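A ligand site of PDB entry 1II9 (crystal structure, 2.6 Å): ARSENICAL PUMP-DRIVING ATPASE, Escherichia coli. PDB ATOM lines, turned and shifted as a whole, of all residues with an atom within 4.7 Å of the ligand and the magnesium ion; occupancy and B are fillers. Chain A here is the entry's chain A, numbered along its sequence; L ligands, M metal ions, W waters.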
ATOM      1  N   GLN A 208      11.189  -2.945  22.721  1.00  0.00           N
ATOM      2  CA  GLN A 208      10.756  -2.854  21.345  1.00  0.00           C
ATOM      3  C   GLN A 208      10.170  -1.454  21.237  1.00  0.00           C
ATOM      4  O   GLN A 208       9.278  -1.108  21.999  1.00  0.00           O
ATOM      5  CB  GLN A 208       9.693  -3.926  21.046  1.00  0.00           C
ATOM      6  CG  GLN A 208       9.467  -4.223  19.563  1.00  0.00           C
ATOM      7  CD  GLN A 208       8.241  -3.545  18.977  1.00  0.00           C
ATOM      8  OE1 GLN A 208       7.115  -3.782  19.403  1.00  0.00           O
ATOM      9  NE2 GLN A 208       8.455  -2.685  17.969  1.00  0.00           N
ATOM     10  N   SER A 210       8.012  -0.007  19.686  1.00  0.00           N
ATOM     11  CA  SER A 210       6.547   0.029  19.695  1.00  0.00           C
ATOM     12  C   SER A 210       5.848  -0.272  21.038  1.00  0.00           C
ATOM     13  O   SER A 210       4.950   0.471  21.454  1.00  0.00           O
ATOM     14  CB  SER A 210       6.023  -0.939  18.630  1.00  0.00           C
ATOM     15  OG  SER A 210       4.619  -0.968  18.606  1.00  0.00           O
ATOM     16  N   ARG A 255      18.942  -3.523  18.308  1.00  0.00           N
ATOM     17  CA  ARG A 255      17.609  -2.950  18.212  1.00  0.00           C
ATOM     18  C   ARG A 255      17.042  -2.631  19.596  1.00  0.00           C
ATOM     19  O   ARG A 255      16.307  -1.644  19.762  1.00  0.00           O
ATOM     20  CB  ARG A 255      16.688  -3.927  17.471  1.00  0.00           C
ATOM     21  CG  ARG A 255      15.346  -3.357  17.091  1.00  0.00           C
ATOM     22  CD  ARG A 255      14.847  -3.995  15.789  1.00  0.00           C
ATOM     23  NE  ARG A 255      14.789  -5.456  15.851  1.00  0.00           N
ATOM     24  CZ  ARG A 255      14.403  -6.227  14.838  1.00  0.00           C
ATOM     25  NH1 ARG A 255      14.042  -5.686  13.685  1.00  0.00           N
ATOM     26  NH2 ARG A 255      14.374  -7.549  14.979  1.00  0.00           N
ATOM     27  N   LYS A 335      -4.813  -8.960  18.353  1.00  0.00           N
ATOM     28  CA  LYS A 335      -4.605  -8.029  19.452  1.00  0.00           C
ATOM     29  C   LYS A 335      -3.643  -6.943  19.023  1.00  0.00           C
ATOM     30  O   LYS A 335      -3.146  -6.944  17.904  1.00  0.00           O
ATOM     31  CB  LYS A 335      -4.041  -8.752  20.687  1.00  0.00           C
ATOM     32  CG  LYS A 335      -4.827  -9.989  21.108  1.00  0.00           C
ATOM     33  CD  LYS A 335      -6.243  -9.659  21.494  1.00  0.00           C
ATOM     34  CE  LYS A 335      -6.282  -8.810  22.758  1.00  0.00           C
ATOM     35  NZ  LYS A 335      -7.668  -8.640  23.277  1.00  0.00           N
ATOM     36  N   GLY A 336      -3.376  -5.998  19.917  1.00  0.00           N
ATOM     37  CA  GLY A 336      -2.472  -4.921  19.593  1.00  0.00           C
ATOM     38  C   GLY A 336      -1.031  -5.373  19.541  1.00  0.00           C
ATOM     39  O   GLY A 336      -0.602  -6.204  20.359  1.00  0.00           O
ATOM     40  N   GLY A 337      -0.315  -4.851  18.550  1.00  0.00           N
ATOM     41  CA  GLY A 337       1.097  -5.156  18.385  1.00  0.00           C
ATOM     42  C   GLY A 337       1.516  -6.483  17.767  1.00  0.00           C
ATOM     43  O   GLY A 337       2.696  -6.646  17.468  1.00  0.00           O
ATOM     44  N   VAL A 338       0.611  -7.428  17.538  1.00  0.00           N
ATOM     45  CA  VAL A 338       1.057  -8.692  16.946  1.00  0.00           C
ATOM     46  C   VAL A 338       1.564  -8.567  15.508  1.00  0.00           C
ATOM     47  O   VAL A 338       2.049  -9.535  14.938  1.00  0.00           O
ATOM     48  CB  VAL A 338      -0.048  -9.771  16.986  1.00  0.00           C
ATOM     49  CG1 VAL A 338      -0.452 -10.019  18.424  1.00  0.00           C
ATOM     50  CG2 VAL A 338      -1.237  -9.338  16.159  1.00  0.00           C
ATOM     51  N   GLY A 339       1.449  -7.372  14.936  1.00  0.00           N
ATOM     52  CA  GLY A 339       1.929  -7.135  13.582  1.00  0.00           C
ATOM     53  C   GLY A 339       0.889  -7.131  12.477  1.00  0.00           C
ATOM     54  O   GLY A 339       1.181  -7.451  11.313  1.00  0.00           O
ATOM     55  N   LYS A 340      -0.340  -6.762  12.816  1.00  0.00           N
ATOM     56  CA  LYS A 340      -1.410  -6.759  11.824  1.00  0.00           C
ATOM     57  C   LYS A 340      -1.063  -5.925  10.609  1.00  0.00           C
ATOM     58  O   LYS A 340      -1.116  -6.414   9.478  1.00  0.00           O
ATOM     59  CB  LYS A 340      -2.728  -6.257  12.446  1.00  0.00           C
ATOM     60  CG  LYS A 340      -3.299  -7.244  13.461  1.00  0.00           C
ATOM     61  CD  LYS A 340      -4.595  -6.776  14.088  1.00  0.00           C
ATOM     62  CE  LYS A 340      -4.456  -5.395  14.681  1.00  0.00           C
ATOM     63  NZ  LYS A 340      -3.330  -5.289  15.621  1.00  0.00           N
ATOM     64  N   THR A 341      -0.678  -4.678  10.833  1.00  0.00           N
ATOM     65  CA  THR A 341      -0.357  -3.779   9.735  1.00  0.00           C
ATOM     66  C   THR A 341       0.784  -4.297   8.843  1.00  0.00           C
ATOM     67  O   THR A 341       0.753  -4.123   7.627  1.00  0.00           O
ATOM     68  CB  THR A 341      -0.103  -2.344  10.294  1.00  0.00           C
ATOM     69  OG1 THR A 341      -1.316  -1.837  10.853  1.00  0.00           O
ATOM     70  CG2 THR A 341       0.355  -1.384   9.221  1.00  0.00           C
ATOM     71  N   THR A 342       1.773  -4.940   9.445  1.00  0.00           N
ATOM     72  CA  THR A 342       2.875  -5.479   8.694  1.00  0.00           C
ATOM     73  C   THR A 342       2.412  -6.672   7.843  1.00  0.00           C
ATOM     74  O   THR A 342       2.777  -6.781   6.669  1.00  0.00           O
ATOM     75  CB  THR A 342       4.008  -5.899   9.620  1.00  0.00           C
ATOM     76  OG1 THR A 342       4.449  -4.755  10.363  1.00  0.00           O
ATOM     77  CG2 THR A 342       5.177  -6.461   8.839  1.00  0.00           C
ATOM     78  N   MET A 343       1.612  -7.570   8.417  1.00  0.00           N
ATOM     79  CA  MET A 343       1.143  -8.719   7.639  1.00  0.00           C
ATOM     80  C   MET A 343       0.243  -8.197   6.513  1.00  0.00           C
ATOM     81  O   MET A 343       0.313  -8.695   5.381  1.00  0.00           O
ATOM     82  CB  MET A 343       0.385  -9.734   8.504  1.00  0.00           C
ATOM     83  CG  MET A 343       1.272 -10.426   9.564  1.00  0.00           C
ATOM     84  SD  MET A 343       2.746 -11.295   8.908  1.00  0.00           S
ATOM     85  CE  MET A 343       3.943 -10.018   8.922  1.00  0.00           C
ATOM     86  N   ASP A 364      -2.493   3.552  10.282  1.00  0.00           N
ATOM     87  CA  ASP A 364      -1.219   3.937  10.891  1.00  0.00           C
ATOM     88  C   ASP A 364      -0.235   4.322   9.772  1.00  0.00           C
ATOM     89  O   ASP A 364      -0.198   3.666   8.731  1.00  0.00           O
ATOM     90  CB  ASP A 364      -0.716   2.747  11.726  1.00  0.00           C
ATOM     91  CG  ASP A 364       0.766   2.788  12.019  1.00  0.00           C
ATOM     92  OD1 ASP A 364       1.300   3.856  12.389  1.00  0.00           O
ATOM     93  OD2 ASP A 364       1.412   1.721  11.890  1.00  0.00           O
ATOM     94  N   ASP A 447      -5.989  -3.677   7.841  1.00  0.00           N
ATOM     95  CA  ASP A 447      -5.130  -4.140   8.935  1.00  0.00           C
ATOM     96  C   ASP A 447      -5.761  -4.194  10.291  1.00  0.00           C
ATOM     97  O   ASP A 447      -5.078  -4.455  11.290  1.00  0.00           O
ATOM     98  CB  ASP A 447      -3.829  -3.332   9.022  1.00  0.00           C
ATOM     99  CG  ASP A 447      -4.065  -1.873   9.384  1.00  0.00           C
ATOM    100  OD1 ASP A 447      -5.178  -1.503   9.808  1.00  0.00           O
ATOM    101  OD2 ASP A 447      -3.109  -1.083   9.236  1.00  0.00           O
ATOM    102  N   ASN A 527       3.379 -14.794  13.711  1.00  0.00           N
ATOM    103  CA  ASN A 527       4.448 -13.833  13.480  1.00  0.00           C
ATOM    104  C   ASN A 527       5.616 -13.877  14.462  1.00  0.00           C
ATOM    105  O   ASN A 527       5.545 -14.488  15.534  1.00  0.00           O
ATOM    106  CB  ASN A 527       3.809 -12.433  13.478  1.00  0.00           C
ATOM    107  CG  ASN A 527       4.699 -11.365  12.857  1.00  0.00           C
ATOM    108  OD1 ASN A 527       5.643 -11.662  12.133  1.00  0.00           O
ATOM    109  ND2 ASN A 527       4.369 -10.123  13.115  1.00  0.00           N
ATOM    110  N   ASN A 528       6.719 -13.220  14.080  1.00  0.00           N
ATOM    111  CA  ASN A 528       7.913 -13.191  14.918  1.00  0.00           C
ATOM    112  C   ASN A 528       8.326 -14.572  15.353  1.00  0.00           C
ATOM    113  O   ASN A 528       8.514 -14.795  16.544  1.00  0.00           O
ATOM    114  CB  ASN A 528       7.662 -12.364  16.188  1.00  0.00           C
ATOM    115  CG  ASN A 528       7.336 -10.934  15.890  1.00  0.00           C
ATOM    116  OD1 ASN A 528       8.155 -10.197  15.343  1.00  0.00           O
ATOM    117  ND2 ASN A 528       6.128 -10.511  16.253  1.00  0.00           N
ATOM    118  N   VAL A 565       5.732 -16.807   9.983  1.00  0.00           N
ATOM    119  CA  VAL A 565       6.588 -15.711   9.583  1.00  0.00           C
ATOM    120  C   VAL A 565       7.750 -15.661  10.577  1.00  0.00           C
ATOM    121  O   VAL A 565       7.594 -16.016  11.747  1.00  0.00           O
ATOM    122  CB  VAL A 565       5.827 -14.358   9.550  1.00  0.00           C
ATOM    123  CG1 VAL A 565       6.711 -13.288   8.950  1.00  0.00           C
ATOM    124  CG2 VAL A 565       4.552 -14.491   8.714  1.00  0.00           C
ATOM    125  N   PRO A 566       8.939 -15.229  10.126  1.00  0.00           N
ATOM    126  CA  PRO A 566      10.073 -15.183  11.043  1.00  0.00           C
ATOM    127  C   PRO A 566      10.338 -13.837  11.661  1.00  0.00           C
ATOM    128  O   PRO A 566       9.883 -12.814  11.143  1.00  0.00           O
ATOM    129  CB  PRO A 566      11.211 -15.586  10.143  1.00  0.00           C
ATOM    130  CG  PRO A 566      10.891 -14.768   8.913  1.00  0.00           C
ATOM    131  CD  PRO A 566       9.396 -15.035   8.742  1.00  0.00           C
ATOM    132  N   VAL A 567      11.083 -13.853  12.765  1.00  0.00           N
ATOM    133  CA  VAL A 567      11.528 -12.653  13.461  1.00  0.00           C
ATOM    134  C   VAL A 567      12.539 -12.119  12.471  1.00  0.00           C
ATOM    135  O   VAL A 567      13.636 -12.656  12.364  1.00  0.00           O
ATOM    136  CB  VAL A 567      12.293 -12.986  14.739  1.00  0.00           C
ATOM    137  CG1 VAL A 567      12.914 -11.736  15.289  1.00  0.00           C
ATOM    138  CG2 VAL A 567      11.365 -13.623  15.759  1.00  0.00           C
ATOM    139  N   LEU A 568      12.192 -11.064  11.742  1.00  0.00           N
ATOM    140  CA  LEU A 568      13.069 -10.524  10.716  1.00  0.00           C
ATOM    141  C   LEU A 568      14.439 -10.057  11.181  1.00  0.00           C
ATOM    142  O   LEU A 568      15.454 -10.374  10.541  1.00  0.00           O
ATOM    143  CB  LEU A 568      12.369  -9.391   9.956  1.00  0.00           C
ATOM    144  CG  LEU A 568      12.789  -9.218   8.479  1.00  0.00           C
ATOM    145  CD1 LEU A 568      11.788  -8.335   7.755  1.00  0.00           C
ATOM    146  CD2 LEU A 568      14.181  -8.618   8.370  1.00  0.00           C
ATOM    147  N   ALA A 569      14.509  -9.326  12.283  1.00  0.00           N
ATOM    148  CA  ALA A 569      15.803  -8.806  12.730  1.00  0.00           C
ATOM    149  C   ALA A 569      16.173  -7.743  11.690  1.00  0.00           C
ATOM    150  O   ALA A 569      17.156  -7.844  10.948  1.00  0.00           O
ATOM    151  CB  ALA A 569      16.849  -9.925  12.747  1.00  0.00           C
ATOM    152  N   SER A 570      15.313  -6.724  11.667  1.00  0.00           N
ATOM    153  CA  SER A 570      15.362  -5.566  10.782  1.00  0.00           C
ATOM    154  C   SER A 570      13.889  -5.179  10.682  1.00  0.00           C
ATOM    155  O   SER A 570      13.042  -6.030  10.451  1.00  0.00           O
ATOM    156  CB  SER A 570      15.896  -5.947   9.394  1.00  0.00           C
ATOM    157  OG  SER A 570      15.913  -4.819   8.549  1.00  0.00           O
ATOM    158  N   GLU A 571      13.578  -3.898  10.886  1.00  0.00           N
ATOM    159  CA  GLU A 571      12.180  -3.463  10.817  1.00  0.00           C
ATOM    160  C   GLU A 571      11.633  -3.524   9.405  1.00  0.00           C
ATOM    161  O   GLU A 571      12.128  -2.821   8.522  1.00  0.00           O
ATOM    162  CB  GLU A 571      12.011  -2.039  11.362  1.00  0.00           C
ATOM    163  CG  GLU A 571      11.099  -1.934  12.579  1.00  0.00           C
ATOM    164  CD  GLU A 571      11.641  -2.711  13.776  1.00  0.00           C
ATOM    165  OE1 GLU A 571      10.987  -2.702  14.838  1.00  0.00           O
ATOM    166  OE2 GLU A 571      12.735  -3.313  13.651  1.00  0.00           O
ATOM    167  N   PRO A 572      10.612  -4.372   9.174  1.00  0.00           N
ATOM    168  CA  PRO A 572       9.978  -4.541   7.869  1.00  0.00           C
ATOM    169  C   PRO A 572       9.370  -3.223   7.402  1.00  0.00           C
ATOM    170  O   PRO A 572       8.176  -3.146   7.116  1.00  0.00           O
ATOM    171  CB  PRO A 572       8.921  -5.602   8.137  1.00  0.00           C
ATOM    172  CG  PRO A 572       9.518  -6.391   9.248  1.00  0.00           C
ATOM    173  CD  PRO A 572      10.059  -5.322  10.149  1.00  0.00           C
ATOM    174  N   LEU A 581       9.575 -11.320   4.483  1.00  0.00           N
ATOM    175  CA  LEU A 581       8.703 -12.028   5.414  1.00  0.00           C
ATOM    176  C   LEU A 581       7.961 -13.185   4.763  1.00  0.00           C
ATOM    177  O   LEU A 581       7.738 -14.234   5.372  1.00  0.00           O
ATOM    178  CB  LEU A 581       7.643 -11.071   6.004  1.00  0.00           C
ATOM    179  CG  LEU A 581       8.123  -9.873   6.813  1.00  0.00           C
ATOM    180  CD1 LEU A 581       6.917  -9.094   7.309  1.00  0.00           C
ATOM    181  CD2 LEU A 581       8.975 -10.337   7.985  1.00  0.00           C
HETATM  182  P1  LIG L   1      -1.551  -2.069  16.158  1.00  0.00           P
HETATM  183  O1  LIG L   1      -2.103  -3.162  17.041  1.00  0.00           O
HETATM  184  O2  LIG L   1      -2.388  -1.681  14.990  1.00  0.00           O
HETATM  185  O3  LIG L   1      -0.841  -0.942  16.836  1.00  0.00           O
HETATM  186  P2  LIG L   1      -0.179  -4.031  14.480  1.00  0.00           P
HETATM  187  O4  LIG L   1      -0.573  -3.363  13.192  1.00  0.00           O
HETATM  188  O5  LIG L   1      -0.606  -5.273  15.198  1.00  0.00           O
HETATM  189  N1  LIG L   1      -0.297  -2.808  15.495  1.00  0.00           N
HETATM  190  P3  LIG L   1       2.686  -3.818  13.642  1.00  0.00           P
HETATM  191  O6  LIG L   1       2.702  -4.528  12.329  1.00  0.00           O
HETATM  192  O7  LIG L   1       2.655  -2.305  13.689  1.00  0.00           O
HETATM  193  O8  LIG L   1       1.409  -4.081  14.555  1.00  0.00           O
HETATM  194  O9  LIG L   1       3.734  -4.492  14.640  1.00  0.00           O
HETATM  195  C1  LIG L   1       4.495  -3.783  15.613  1.00  0.00           C
HETATM  196  C2  LIG L   1       5.934  -3.587  15.157  1.00  0.00           C
HETATM  197  O10 LIG L   1       6.649  -4.841  15.082  1.00  0.00           O
HETATM  198  C3  LIG L   1       6.315  -2.880  13.857  1.00  0.00           C
HETATM  199  O11 LIG L   1       7.121  -1.749  14.160  1.00  0.00           O
HETATM  200  C4  LIG L   1       7.092  -3.840  12.984  1.00  0.00           C
HETATM  201  O12 LIG L   1       8.088  -3.515  12.024  1.00  0.00           O
HETATM  202  C5  LIG L   1       7.457  -4.962  13.935  1.00  0.00           C
HETATM  203  N2  LIG L   1       7.146  -6.263  13.355  1.00  0.00           N
HETATM  204  C6  LIG L   1       5.936  -6.810  12.978  1.00  0.00           C
HETATM  205  N3  LIG L   1       6.081  -7.994  12.439  1.00  0.00           N
HETATM  206  C7  LIG L   1       7.445  -8.251  12.475  1.00  0.00           C
HETATM  207  C8  LIG L   1       8.339  -9.288  12.078  1.00  0.00           C
HETATM  208  N4  LIG L   1       7.899 -10.393  11.473  1.00  0.00           N
HETATM  209  N5  LIG L   1       9.696  -9.221  12.295  1.00  0.00           N
HETATM  210  C9  LIG L   1      10.274  -8.143  12.892  1.00  0.00           C
HETATM  211  N6  LIG L   1       9.482  -7.126  13.273  1.00  0.00           N
HETATM  212  C10 LIG L   1       8.129  -7.184  13.071  1.00  0.00           C
HETATM  213 MG    MG M   1      -1.665  -1.635  13.080  1.00  0.00          MG
HETATM  214  O   HOH W   1      -5.363  -1.278  14.791  1.00  0.00           O
HETATM  215  O   HOH W   2      -2.609   0.150  12.342  1.00  0.00           O
HETATM  216  O   HOH W   3       2.145  -1.633  17.217  1.00  0.00           O
HETATM  217  O   HOH W   4       6.173  -2.467  10.183  1.00  0.00           O
HETATM  218  O   HOH W   5      -3.334  -2.652  12.734  1.00  0.00           O
HETATM  219  O   HOH W   6       0.103  -0.747  13.150  1.00  0.00           O
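NH1 of Arg 255 is in salt-bridge range of OE2 of Glu 571.
The side-chain carboxylate of Asp 447 lies close to the side-chain hydroxyl of Thr 341.
NZ of Lys 340 sits at hydrogen-bond distance from O of Lys 335, 2.8 Å away.
The side-chain amide nitrogen (NE2) of Gln 208 sits close to the backbone NH (N) of Ser 210 (3.2 Å).
The side-chain amide nitrogen (ND2) of Asn 527 lies within hydrogen-bond range of the backbone carbonyl oxygen (O) of Val 338, at 3.0 Å.
N of Thr 341 sits close to O4 of the ligand, at 2.7 Å.
The backbone NH of Val 338 lies within hydrogen-bond range of an oxygen (O5) of the ligand, at 3.4 Å.
The backbone NH of Thr 342 sits at hydrogen-bond distance from an oxygen (O6) of the ligand, at 3.1 Å.
The side-chain amino group (NZ) of Lys 340 lies within salt-bridge range of an oxygen (O5) of the ligand, 2.8 Å away.
N4 of the ligand lies within hydrogen-bond range of O of Pro 566, 3.1 Å away.
An oxygen (O5) of the ligand sits at hydrogen-bond distance from the backbone NH (N) of Lys 340, 2.8 Å away.
The backbone NH (N) of Leu 568 lies within hydrogen-bond range of a nitrogen (N5) of the ligand, 3.2 Å away.
OD1 of Asn 527 is in hydrogen-bond range of N4 of the ligand (2.7 Å).
The side-chain hydroxyl of Thr 342 sits at hydrogen-bond distance from an oxygen (O6) of the ligand.
The backbone NH (N) of Gly 337 is in hydrogen-bond range of an oxygen (O1) of the ligand, 2.9 Å away.
N of Gly 339 is in hydrogen-bond range of O5 of the ligand (2.9 Å).
Within 4 Å of the magnesium ion: Thr 341.
Water W6 lies within hydrogen-bond range of an oxygen (O7) of the ligand (3.0 Å) and the side-chain carboxylate (OD2) of Asp 364 (3.1 Å).
Water W4 bridges an oxygen (O12) of the ligand (2.9 Å) and the side-chain hydroxyl of Thr 342 (2.9 Å).
Water W3 bridges the side-chain hydroxyl of Ser 210 (2.9 Å) and an oxygen (O3) of the ligand (3.1 Å).
Residues that only touch the ligand: Gln 208 (3.9 Å), Gly 336 (3.1 Å), Asn 528 (3.4 Å), Glu 571 (3.4 Å), Pro 572 (3.3 Å) and Leu 581 (3.7 Å).
Hydrophobic or aromatic side chains within 4 Å of the ligand: Leu 568, Pro 572 and Leu 581.
Within 4 Å of the ligand: Gln 208, Gly 336, Gly 337, Val 338, Gly 339, Lys 340, Thr 341, Thr 342, Asn 527, Asn 528, Pro 566, Leu 568, Glu 571, Pro 572 and Leu 581.
The magnesium ion is bound by water W6 (2.0 Å), water W5 (2.0 Å), O2 of the ligand (2.0 Å), O4 of the ligand (2.0 Å), water W2 (2.1 Å) and OG1 of Thr 341 (2.3 Å).
The magnesium ion has six donor atoms within binding distance.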
